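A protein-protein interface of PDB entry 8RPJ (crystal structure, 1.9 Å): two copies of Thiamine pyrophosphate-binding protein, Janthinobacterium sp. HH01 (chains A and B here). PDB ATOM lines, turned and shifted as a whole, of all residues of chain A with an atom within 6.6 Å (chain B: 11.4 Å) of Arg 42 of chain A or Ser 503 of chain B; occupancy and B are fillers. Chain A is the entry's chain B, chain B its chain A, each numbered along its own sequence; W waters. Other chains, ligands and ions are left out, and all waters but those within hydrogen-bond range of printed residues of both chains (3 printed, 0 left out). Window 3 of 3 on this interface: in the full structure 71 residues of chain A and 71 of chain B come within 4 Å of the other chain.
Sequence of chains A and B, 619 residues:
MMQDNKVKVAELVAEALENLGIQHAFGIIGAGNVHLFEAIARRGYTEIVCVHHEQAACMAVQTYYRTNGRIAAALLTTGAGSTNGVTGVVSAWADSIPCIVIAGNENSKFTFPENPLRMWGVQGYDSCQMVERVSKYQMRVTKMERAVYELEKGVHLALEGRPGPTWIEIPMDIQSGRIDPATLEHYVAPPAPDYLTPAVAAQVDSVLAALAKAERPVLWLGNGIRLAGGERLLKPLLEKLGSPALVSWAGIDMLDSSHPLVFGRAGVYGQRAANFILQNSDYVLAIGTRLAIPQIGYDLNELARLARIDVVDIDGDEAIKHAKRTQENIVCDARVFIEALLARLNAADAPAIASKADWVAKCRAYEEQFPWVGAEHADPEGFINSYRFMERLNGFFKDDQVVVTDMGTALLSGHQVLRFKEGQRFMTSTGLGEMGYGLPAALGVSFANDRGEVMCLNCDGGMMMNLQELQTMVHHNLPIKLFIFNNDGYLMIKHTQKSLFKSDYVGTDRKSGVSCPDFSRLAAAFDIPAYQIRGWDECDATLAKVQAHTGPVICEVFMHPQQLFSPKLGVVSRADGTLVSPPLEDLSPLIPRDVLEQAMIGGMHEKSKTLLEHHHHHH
OG of Ser 503 of chain B lies within hydrogen-bond range of OE2 of Glu 38 of chain A (3.2 Å).
OG of Ser 503 of chain B lies within hydrogen-bond range of NH2 of Arg 42 of chain A, 2.8 Å away.
The backbone carbonyl oxygen of Asp 504 of chain B is in hydrogen-bond range of the guanidinium group of Arg 42 of chain A (2.8 Å).
The side-chain amide nitrogen (NE2) of Gln 497 of chain B lies within hydrogen-bond range of the backbone carbonyl oxygen (O) of Val 506 of chain B, at 3.1 Å.
NZ of Lys 498 of chain B lies within hydrogen-bond range of O of Ser 503 of chain B.
The side-chain carboxylate (OE2) of Glu 38 of chain A is in salt-bridge range of the guanidinium group (NH2) of Arg 42 of chain A (2.9 Å).
Among the printed residues, pairs that only touch across the chains: Glu 38 of chain A with Phe 501 of chain B (3.4 Å), Ala 41 of chain A with Val 506 of chain B (3.5 Å), Glu 38 of chain A with Val 506 of chain B (3.6 Å), Arg 42 of chain A with Val 506 of chain B (3.7 Å) and Phe 37 of chain A with Val 506 of chain B (3.8 Å).
Printed residues of chain B within 4 Å of Phe 37 of chain A: Val 506.
Glu 38 of chain A touches just these residues of chain B: Phe 501 (3.4 Å), Ser 503 (3.2 Å) and Val 506 (3.6 Å).
No residue of chain B comes within 4 Å of Ala 39 of chain A.
Ala 41 of chain A touches just one residue of chain B: Val 506.
Of chain B, only Ser 503, Asp 504 and Val 506 come within 4 Å of Arg 42 of chain A.
Arg 43 of chain A touches none of the printed residues of chain B.
No residue of chain B comes within 4 Å of Gly 44 of chain A.
Ser 503 of chain B touches just these residues of chain A: Glu 38 (3.2 Å) and Arg 42 (2.8 Å).
Printed residues of chain A within 4 Å of Val 506 of chain B: Phe 37, Glu 38, Ala 41 and Arg 42.
The nearest printed residue of chain A that does not touch Ser 503 of chain B is Ala 41 of chain A (8.5 Å).
The nearest printed residue of chain A that does not touch Asp 504 of chain B is Glu 38 of chain A (4.6 Å).
Printed residues of chain B that touch a printed residue of chain A: Phe 501, Ser 503, Asp 504 and Val 506.
Hydrophobic or aromatic side chains of chain B that line the printed part of chain A: Phe 501 and Val 506.
Of the 10 printed residues of chain A, 4 touch a printed residue of chain B.
Printed residues of chain A that touch a printed residue of chain B: Phe 37, Glu 38, Ala 41 and Arg 42.
Hydrophobic or aromatic side chains of chain A within 4 Å of the printed part of chain B: Ala 41.
Along chain A the printed residues that touch a printed residue of chain B span positions 37 to 42.
No position is printed for both chains.
Of the 8 pairs that touch across the chains among the printed residues, none has its exchanged pair printed and touching as well.
Water W2 bridges the backbone carbonyl oxygen of Asp 504 of chain B (2.7 Å) and the side-chain carboxylate of Glu 38 of chain A (2.8 Å).
Water W1 lies within hydrogen-bond range of OE1 of Glu 38 of chain A and NE2 of Gln 497 of chain B.
Water W3 lies within hydrogen-bond range of OE2 of Glu 38 of chain A and OG of Ser 503 of chain B.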
ATOM      1  N   GLU A  11      34.353 -14.149  29.542  1.00  0.00           N
ATOM      2  CA  GLU A  11      34.295 -13.523  30.857  1.00  0.00           C
ATOM      3  C   GLU A  11      35.584 -12.775  31.168  1.00  0.00           C
ATOM      4  O   GLU A  11      35.554 -11.701  31.782  1.00  0.00           O
ATOM      5  CB  GLU A  11      34.007 -14.586  31.913  1.00  0.00           C
ATOM      6  CG  GLU A  11      32.626 -15.192  31.756  1.00  0.00           C
ATOM      7  CD  GLU A  11      32.357 -16.323  32.714  1.00  0.00           C
ATOM      8  OE1 GLU A  11      33.163 -17.276  32.767  1.00  0.00           O
ATOM      9  OE2 GLU A  11      31.330 -16.257  33.425  1.00  0.00           O
ATOM     10  N   PHE A  37      28.579 -10.430  24.237  1.00  0.00           N
ATOM     11  CA  PHE A  37      27.409  -9.724  24.745  1.00  0.00           C
ATOM     12  C   PHE A  37      26.981 -10.305  26.082  1.00  0.00           C
ATOM     13  O   PHE A  37      26.680  -9.569  27.028  1.00  0.00           O
ATOM     14  CB  PHE A  37      26.247  -9.801  23.754  1.00  0.00           C
ATOM     15  CG  PHE A  37      26.158  -8.631  22.811  1.00  0.00           C
ATOM     16  CD1 PHE A  37      27.112  -8.445  21.831  1.00  0.00           C
ATOM     17  CD2 PHE A  37      25.104  -7.731  22.891  1.00  0.00           C
ATOM     18  CE1 PHE A  37      27.027  -7.380  20.952  1.00  0.00           C
ATOM     19  CE2 PHE A  37      25.011  -6.665  22.013  1.00  0.00           C
ATOM     20  CZ  PHE A  37      25.977  -6.488  21.039  1.00  0.00           C
ATOM     21  N   GLU A  38      26.949 -11.633  26.180  1.00  0.00           N
ATOM     22  CA  GLU A  38      26.477 -12.258  27.405  1.00  0.00           C
ATOM     23  C   GLU A  38      27.397 -11.923  28.569  1.00  0.00           C
ATOM     24  O   GLU A  38      26.941 -11.493  29.635  1.00  0.00           O
ATOM     25  CB  GLU A  38      26.374 -13.769  27.220  1.00  0.00           C
ATOM     26  CG  GLU A  38      25.625 -14.458  28.343  1.00  0.00           C
ATOM     27  CD  GLU A  38      24.137 -14.150  28.333  1.00  0.00           C
ATOM     28  OE1 GLU A  38      23.645 -13.607  27.324  1.00  0.00           O
ATOM     29  OE2 GLU A  38      23.461 -14.455  29.339  1.00  0.00           O
ATOM     30  N   ALA A  39      28.705 -12.101  28.371  1.00  0.00           N
ATOM     31  CA  ALA A  39      29.663 -11.891  29.448  1.00  0.00           C
ATOM     32  C   ALA A  39      29.664 -10.445  29.918  1.00  0.00           C
ATOM     33  O   ALA A  39      29.722 -10.173  31.123  1.00  0.00           O
ATOM     34  CB  ALA A  39      31.061 -12.292  28.975  1.00  0.00           C
ATOM     35  N   ILE A  40      29.627  -9.506  28.975  1.00  0.00           N
ATOM     36  CA  ILE A  40      29.642  -8.092  29.328  1.00  0.00           C
ATOM     37  C   ILE A  40      28.370  -7.727  30.071  1.00  0.00           C
ATOM     38  O   ILE A  40      28.404  -7.009  31.077  1.00  0.00           O
ATOM     39  CB  ILE A  40      29.824  -7.237  28.058  1.00  0.00           C
ATOM     40  CG1 ILE A  40      31.217  -7.450  27.460  1.00  0.00           C
ATOM     41  CG2 ILE A  40      29.577  -5.773  28.377  1.00  0.00           C
ATOM     42  CD1 ILE A  40      31.404  -6.815  26.087  1.00  0.00           C
ATOM     43  N   ALA A  41      27.226  -8.211  29.586  1.00  0.00           N
ATOM     44  CA  ALA A  41      25.961  -7.889  30.228  1.00  0.00           C
ATOM     45  C   ALA A  41      25.915  -8.428  31.652  1.00  0.00           C
ATOM     46  O   ALA A  41      25.404  -7.762  32.559  1.00  0.00           O
ATOM     47  CB  ALA A  41      24.803  -8.446  29.405  1.00  0.00           C
ATOM     48  N   ARG A  42      26.439  -9.638  31.870  1.00  0.00           N
ATOM     49  CA  ARG A  42      26.340 -10.236  33.196  1.00  0.00           C
ATOM     50  C   ARG A  42      27.280  -9.558  34.186  1.00  0.00           C
ATOM     51  O   ARG A  42      26.960  -9.462  35.376  1.00  0.00           O
ATOM     52  CB  ARG A  42      26.632 -11.740  33.141  1.00  0.00           C
ATOM     53  CG  ARG A  42      25.586 -12.594  32.402  1.00  0.00           C
ATOM     54  CD  ARG A  42      24.128 -12.218  32.721  1.00  0.00           C
ATOM     55  NE  ARG A  42      23.184 -12.892  31.832  1.00  0.00           N
ATOM     56  CZ  ARG A  42      22.004 -12.408  31.468  1.00  0.00           C
ATOM     57  NH1 ARG A  42      21.578 -11.233  31.887  1.00  0.00           N
ATOM     58  NH2 ARG A  42      21.235 -13.119  30.652  1.00  0.00           N
ATOM     59  N   ARG A  43      28.434  -9.082  33.720  1.00  0.00           N
ATOM     60  CA  ARG A  43      29.345  -8.378  34.615  1.00  0.00           C
ATOM     61  C   ARG A  43      28.751  -7.046  35.059  1.00  0.00           C
ATOM     62  O   ARG A  43      28.879  -6.661  36.226  1.00  0.00           O
ATOM     63  CB  ARG A  43      30.694  -8.172  33.934  1.00  0.00           C
ATOM     64  CG  ARG A  43      31.722  -7.550  34.850  1.00  0.00           C
ATOM     65  CD  ARG A  43      33.127  -7.717  34.318  1.00  0.00           C
ATOM     66  NE  ARG A  43      34.106  -7.301  35.319  1.00  0.00           N
ATOM     67  CZ  ARG A  43      34.680  -8.119  36.195  1.00  0.00           C
ATOM     68  NH1 ARG A  43      34.474  -9.424  36.161  1.00  0.00           N
ATOM     69  NH2 ARG A  43      35.480  -7.611  37.130  1.00  0.00           N
ATOM     70  N   GLY A  44      28.104  -6.327  34.145  1.00  0.00           N
ATOM     71  CA  GLY A  44      27.400  -5.115  34.501  1.00  0.00           C
ATOM     72  C   GLY A  44      28.236  -3.860  34.627  1.00  0.00           C
ATOM     73  O   GLY A  44      27.732  -2.859  35.147  1.00  0.00           O
ATOM     74  N   TYR A  45      29.485  -3.862  34.161  1.00  0.00           N
ATOM     75  CA  TYR A  45      30.291  -2.648  34.230  1.00  0.00           C
ATOM     76  C   TYR A  45      30.191  -1.817  32.958  1.00  0.00           C
ATOM     77  O   TYR A  45      30.006  -0.595  33.013  1.00  0.00           O
ATOM     78  CB  TYR A  45      31.761  -2.995  34.489  1.00  0.00           C
ATOM     79  CG  TYR A  45      32.664  -1.783  34.516  1.00  0.00           C
ATOM     80  CD1 TYR A  45      32.831  -1.056  35.681  1.00  0.00           C
ATOM     81  CD2 TYR A  45      33.338  -1.357  33.374  1.00  0.00           C
ATOM     82  CE1 TYR A  45      33.646   0.055  35.722  1.00  0.00           C
ATOM     83  CE2 TYR A  45      34.157  -0.243  33.402  1.00  0.00           C
ATOM     84  CZ  TYR A  45      34.308   0.457  34.582  1.00  0.00           C
ATOM     85  OH  TYR A  45      35.117   1.567  34.640  1.00  0.00           O
ATOM     86  N   ILE B 493      18.209 -14.457  17.208  1.00  0.00           N
ATOM     87  CA  ILE B 493      19.245 -14.433  18.234  1.00  0.00           C
ATOM     88  C   ILE B 493      18.658 -14.761  19.608  1.00  0.00           C
ATOM     89  O   ILE B 493      19.350 -15.339  20.455  1.00  0.00           O
ATOM     90  CB  ILE B 493      19.971 -13.079  18.230  1.00  0.00           C
ATOM     91  CG1 ILE B 493      20.475 -12.730  16.821  1.00  0.00           C
ATOM     92  CG2 ILE B 493      21.140 -13.110  19.211  1.00  0.00           C
ATOM     93  CD1 ILE B 493      21.407 -13.759  16.185  1.00  0.00           C
ATOM     94  N   LYS B 494      17.388 -14.428  19.853  1.00  0.00           N
ATOM     95  CA  LYS B 494      16.736 -14.897  21.075  1.00  0.00           C
ATOM     96  C   LYS B 494      16.901 -16.408  21.220  1.00  0.00           C
ATOM     97  O   LYS B 494      17.242 -16.911  22.293  1.00  0.00           O
ATOM     98  CB  LYS B 494      15.250 -14.536  21.079  1.00  0.00           C
ATOM     99  CG  LYS B 494      14.958 -13.059  21.199  1.00  0.00           C
ATOM    100  CD  LYS B 494      13.463 -12.838  21.308  1.00  0.00           C
ATOM    101  CE  LYS B 494      13.060 -11.517  20.685  1.00  0.00           C
ATOM    102  NZ  LYS B 494      11.634 -11.213  20.967  1.00  0.00           N
ATOM    103  N   HIS B 495      16.674 -17.148  20.138  1.00  0.00           N
ATOM    104  CA  HIS B 495      16.824 -18.599  20.196  1.00  0.00           C
ATOM    105  C   HIS B 495      18.268 -18.997  20.427  1.00  0.00           C
ATOM    106  O   HIS B 495      18.547 -19.877  21.249  1.00  0.00           O
ATOM    107  CB  HIS B 495      16.286 -19.223  18.913  1.00  0.00           C
ATOM    108  CG  HIS B 495      14.810 -19.065  18.766  1.00  0.00           C
ATOM    109  ND1 HIS B 495      13.943 -19.318  19.804  1.00  0.00           N
ATOM    110  CD2 HIS B 495      14.047 -18.648  17.729  1.00  0.00           C
ATOM    111  CE1 HIS B 495      12.707 -19.080  19.410  1.00  0.00           C
ATOM    112  NE2 HIS B 495      12.741 -18.675  18.153  1.00  0.00           N
ATOM    113  N   THR B 496      19.201 -18.359  19.721  1.00  0.00           N
ATOM    114  CA  THR B 496      20.609 -18.654  19.950  1.00  0.00           C
ATOM    115  C   THR B 496      20.968 -18.475  21.419  1.00  0.00           C
ATOM    116  O   THR B 496      21.516 -19.386  22.051  1.00  0.00           O
ATOM    117  CB  THR B 496      21.485 -17.765  19.076  1.00  0.00           C
ATOM    118  OG1 THR B 496      21.054 -17.861  17.709  1.00  0.00           O
ATOM    119  CG2 THR B 496      22.943 -18.192  19.169  1.00  0.00           C
ATOM    120  N   GLN B 497      20.672 -17.309  21.988  1.00  0.00           N
ATOM    121  CA  GLN B 497      21.172 -17.067  23.337  1.00  0.00           C
ATOM    122  C   GLN B 497      20.396 -17.878  24.371  1.00  0.00           C
ATOM    123  O   GLN B 497      20.986 -18.306  25.369  1.00  0.00           O
ATOM    124  CB  GLN B 497      21.182 -15.570  23.653  1.00  0.00           C
ATOM    125  CG  GLN B 497      19.859 -14.864  23.663  1.00  0.00           C
ATOM    126  CD  GLN B 497      19.967 -13.339  23.736  1.00  0.00           C
ATOM    127  OE1 GLN B 497      18.945 -12.660  23.811  1.00  0.00           O
ATOM    128  NE2 GLN B 497      21.187 -12.802  23.709  1.00  0.00           N
ATOM    129  N   LYS B 498      19.117 -18.176  24.120  1.00  0.00           N
ATOM    130  CA  LYS B 498      18.376 -19.046  25.032  1.00  0.00           C
ATOM    131  C   LYS B 498      18.937 -20.467  25.021  1.00  0.00           C
ATOM    132  O   LYS B 498      19.000 -21.121  26.070  1.00  0.00           O
ATOM    133  CB  LYS B 498      16.896 -19.058  24.658  1.00  0.00           C
ATOM    134  CG  LYS B 498      15.959 -19.229  25.839  1.00  0.00           C
ATOM    135  CD  LYS B 498      15.978 -17.986  26.697  1.00  0.00           C
ATOM    136  CE  LYS B 498      14.988 -18.073  27.834  1.00  0.00           C
ATOM    137  NZ  LYS B 498      14.950 -16.776  28.556  1.00  0.00           N
ATOM    138  N   SER B 499      19.341 -20.963  23.845  1.00  0.00           N
ATOM    139  CA  SER B 499      19.910 -22.308  23.757  1.00  0.00           C
ATOM    140  C   SER B 499      21.226 -22.402  24.519  1.00  0.00           C
ATOM    141  O   SER B 499      21.522 -23.429  25.147  1.00  0.00           O
ATOM    142  CB  SER B 499      20.143 -22.696  22.298  1.00  0.00           C
ATOM    143  OG  SER B 499      18.959 -22.595  21.525  1.00  0.00           O
ATOM    144  N   LEU B 500      22.037 -21.340  24.458  1.00  0.00           N
ATOM    145  CA  LEU B 500      23.350 -21.353  25.085  1.00  0.00           C
ATOM    146  C   LEU B 500      23.289 -21.075  26.584  1.00  0.00           C
ATOM    147  O   LEU B 500      24.049 -21.673  27.354  1.00  0.00           O
ATOM    148  CB  LEU B 500      24.255 -20.309  24.428  1.00  0.00           C
ATOM    149  CG  LEU B 500      24.614 -20.516  22.958  1.00  0.00           C
ATOM    150  CD1 LEU B 500      25.153 -19.205  22.382  1.00  0.00           C
ATOM    151  CD2 LEU B 500      25.616 -21.641  22.789  1.00  0.00           C
ATOM    152  N   PHE B 501      22.423 -20.150  27.015  1.00  0.00           N
ATOM    153  CA  PHE B 501      22.502 -19.621  28.370  1.00  0.00           C
ATOM    154  C   PHE B 501      21.251 -19.818  29.207  1.00  0.00           C
ATOM    155  O   PHE B 501      21.344 -19.745  30.438  1.00  0.00           O
ATOM    156  CB  PHE B 501      22.823 -18.115  28.339  1.00  0.00           C
ATOM    157  CG  PHE B 501      23.965 -17.763  27.438  1.00  0.00           C
ATOM    158  CD1 PHE B 501      25.225 -18.293  27.654  1.00  0.00           C
ATOM    159  CD2 PHE B 501      23.782 -16.902  26.373  1.00  0.00           C
ATOM    160  CE1 PHE B 501      26.276 -17.975  26.821  1.00  0.00           C
ATOM    161  CE2 PHE B 501      24.829 -16.579  25.539  1.00  0.00           C
ATOM    162  CZ  PHE B 501      26.080 -17.116  25.761  1.00  0.00           C
ATOM    163  N   LYS B 502      20.094 -20.038  28.589  1.00  0.00           N
ATOM    164  CA  LYS B 502      18.857 -20.287  29.320  1.00  0.00           C
ATOM    165  C   LYS B 502      18.618 -19.228  30.392  1.00  0.00           C
ATOM    166  O   LYS B 502      18.176 -19.529  31.505  1.00  0.00           O
ATOM    167  CB  LYS B 502      18.868 -21.691  29.925  1.00  0.00           C
ATOM    168  CG  LYS B 502      18.836 -22.782  28.869  1.00  0.00           C
ATOM    169  CD  LYS B 502      18.980 -24.173  29.458  1.00  0.00           C
ATOM    170  CE  LYS B 502      18.430 -25.225  28.497  1.00  0.00           C
ATOM    171  NZ  LYS B 502      18.710 -24.913  27.064  1.00  0.00           N
ATOM    172  N   SER B 503      18.895 -17.975  30.049  1.00  0.00           N
ATOM    173  CA  SER B 503      18.688 -16.867  30.971  1.00  0.00           C
ATOM    174  C   SER B 503      17.966 -15.737  30.239  1.00  0.00           C
ATOM    175  O   SER B 503      17.317 -15.932  29.205  1.00  0.00           O
ATOM    176  CB  SER B 503      20.025 -16.414  31.580  1.00  0.00           C
ATOM    177  OG  SER B 503      20.905 -15.939  30.575  1.00  0.00           O
ATOM    178  N   ASP B 504      18.062 -14.525  30.784  1.00  0.00           N
ATOM    179  CA  ASP B 504      17.322 -13.406  30.221  1.00  0.00           C
ATOM    180  C   ASP B 504      17.954 -12.943  28.916  1.00  0.00           C
ATOM    181  O   ASP B 504      19.170 -13.036  28.719  1.00  0.00           O
ATOM    182  CB  ASP B 504      17.269 -12.232  31.196  1.00  0.00           C
ATOM    183  CG  ASP B 504      16.222 -12.413  32.268  1.00  0.00           C
ATOM    184  OD1 ASP B 504      15.222 -13.120  32.025  1.00  0.00           O
ATOM    185  OD2 ASP B 504      16.400 -11.832  33.359  1.00  0.00           O
ATOM    186  N   TYR B 505      17.112 -12.431  28.021  1.00  0.00           N
ATOM    187  CA  TYR B 505      17.598 -11.940  26.749  1.00  0.00           C
ATOM    188  C   TYR B 505      18.537 -10.757  26.961  1.00  0.00           C
ATOM    189  O   TYR B 505      18.409  -9.995  27.923  1.00  0.00           O
ATOM    190  CB  TYR B 505      16.429 -11.543  25.865  1.00  0.00           C
ATOM    191  CG  TYR B 505      15.580 -12.721  25.439  1.00  0.00           C
ATOM    192  CD1 TYR B 505      16.155 -13.874  24.923  1.00  0.00           C
ATOM    193  CD2 TYR B 505      14.203 -12.675  25.563  1.00  0.00           C
ATOM    194  CE1 TYR B 505      15.379 -14.950  24.532  1.00  0.00           C
ATOM    195  CE2 TYR B 505      13.417 -13.741  25.179  1.00  0.00           C
ATOM    196  CZ  TYR B 505      14.004 -14.875  24.665  1.00  0.00           C
ATOM    197  OH  TYR B 505      13.208 -15.929  24.286  1.00  0.00           O
ATOM    198  N   VAL B 506      19.495 -10.627  26.048  1.00  0.00           N
ATOM    199  CA  VAL B 506      20.514  -9.578  26.079  1.00  0.00           C
ATOM    200  C   VAL B 506      20.656  -9.024  24.669  1.00  0.00           C
ATOM    201  O   VAL B 506      21.050  -9.754  23.751  1.00  0.00           O
ATOM    202  CB  VAL B 506      21.871 -10.112  26.578  1.00  0.00           C
ATOM    203  CG1 VAL B 506      22.955  -9.054  26.441  1.00  0.00           C
ATOM    204  CG2 VAL B 506      21.764 -10.597  28.021  1.00  0.00           C
ATOM    205  N   GLY B 507      20.331  -7.744  24.490  1.00  0.00           N
ATOM    206  CA  GLY B 507      20.553  -7.103  23.208  1.00  0.00           C
ATOM    207  C   GLY B 507      19.678  -7.612  22.084  1.00  0.00           C
ATOM    208  O   GLY B 507      20.055  -7.502  20.912  1.00  0.00           O
ATOM    209  N   THR B 508      18.507  -8.153  22.409  1.00  0.00           N
ATOM    210  CA  THR B 508      17.665  -8.762  21.399  1.00  0.00           C
ATOM    211  C   THR B 508      16.188  -8.399  21.494  1.00  0.00           C
ATOM    212  O   THR B 508      15.419  -8.853  20.644  1.00  0.00           O
ATOM    213  CB  THR B 508      17.782 -10.292  21.472  1.00  0.00           C
ATOM    214  OG1 THR B 508      17.511 -10.719  22.813  1.00  0.00           O
ATOM    215  CG2 THR B 508      19.169 -10.759  21.075  1.00  0.00           C
ATOM    216  N   ASP B 509      15.753  -7.635  22.496  1.00  0.00           N
ATOM    217  CA  ASP B 509      14.354  -7.217  22.566  1.00  0.00           C
ATOM    218  C   ASP B 509      14.269  -5.888  23.314  1.00  0.00           C
ATOM    219  O   ASP B 509      15.278  -5.349  23.775  1.00  0.00           O
ATOM    220  CB  ASP B 509      13.458  -8.314  23.170  1.00  0.00           C
ATOM    221  CG  ASP B 509      13.665  -8.562  24.680  1.00  0.00           C
ATOM    222  OD1 ASP B 509      14.476  -7.889  25.354  1.00  0.00           O
ATOM    223  OD2 ASP B 509      12.970  -9.470  25.182  1.00  0.00           O
ATOM    224  N   LYS B 511      13.185  -4.818  26.174  1.00  0.00           N
ATOM    225  CA  LYS B 511      13.668  -4.732  27.545  1.00  0.00           C
ATOM    226  C   LYS B 511      15.172  -4.935  27.642  1.00  0.00           C
ATOM    227  O   LYS B 511      15.777  -4.480  28.621  1.00  0.00           O
ATOM    228  CB  LYS B 511      12.926  -5.739  28.419  1.00  0.00           C
ATOM    229  CG  LYS B 511      11.506  -5.295  28.755  1.00  0.00           C
ATOM    230  CD  LYS B 511      10.775  -6.288  29.644  1.00  0.00           C
ATOM    231  CE  LYS B 511      11.523  -6.539  30.945  1.00  0.00           C
ATOM    232  NZ  LYS B 511      10.690  -7.278  31.933  1.00  0.00           N
ATOM    233  N   SER B 512      15.796  -5.577  26.648  1.00  0.00           N
ATOM    234  CA  SER B 512      17.229  -5.843  26.697  1.00  0.00           C
ATOM    235  C   SER B 512      18.027  -4.991  25.710  1.00  0.00           C
ATOM    236  O   SER B 512      19.188  -5.308  25.422  1.00  0.00           O
ATOM    237  CB  SER B 512      17.508  -7.330  26.464  1.00  0.00           C
ATOM    238  OG  SER B 512      17.070  -7.758  25.183  1.00  0.00           O
ATOM    239  N   GLY B 513      17.438  -3.917  25.191  1.00  0.00           N
ATOM    240  CA  GLY B 513      18.211  -2.865  24.550  1.00  0.00           C
ATOM    241  C   GLY B 513      17.871  -2.571  23.101  1.00  0.00           C
ATOM    242  O   GLY B 513      18.417  -1.605  22.548  1.00  0.00           O
ATOM    243  N   GLN B 562       8.370 -14.974  20.900  1.00  0.00           N
ATOM    244  CA  GLN B 562       9.297 -16.073  21.142  1.00  0.00           C
ATOM    245  C   GLN B 562       8.988 -17.286  20.271  1.00  0.00           C
ATOM    246  O   GLN B 562       9.365 -18.409  20.627  1.00  0.00           O
ATOM    247  CB  GLN B 562       9.281 -16.468  22.614  1.00  0.00           C
ATOM    248  CG  GLN B 562       9.742 -15.361  23.518  1.00  0.00           C
ATOM    249  CD  GLN B 562       9.693 -15.747  24.969  1.00  0.00           C
ATOM    250  OE1 GLN B 562       8.651 -15.648  25.614  1.00  0.00           O
ATOM    251  NE2 GLN B 562      10.821 -16.210  25.494  1.00  0.00           N
HETATM  252  O   HOH W   1      24.070 -13.048  24.613  1.00  0.00           O
HETATM  253  O   HOH W   2      20.928 -14.238  27.029  1.00  0.00           O
HETATM  254  O   HOH W   3      24.185 -16.363  31.445  1.00  0.00           O
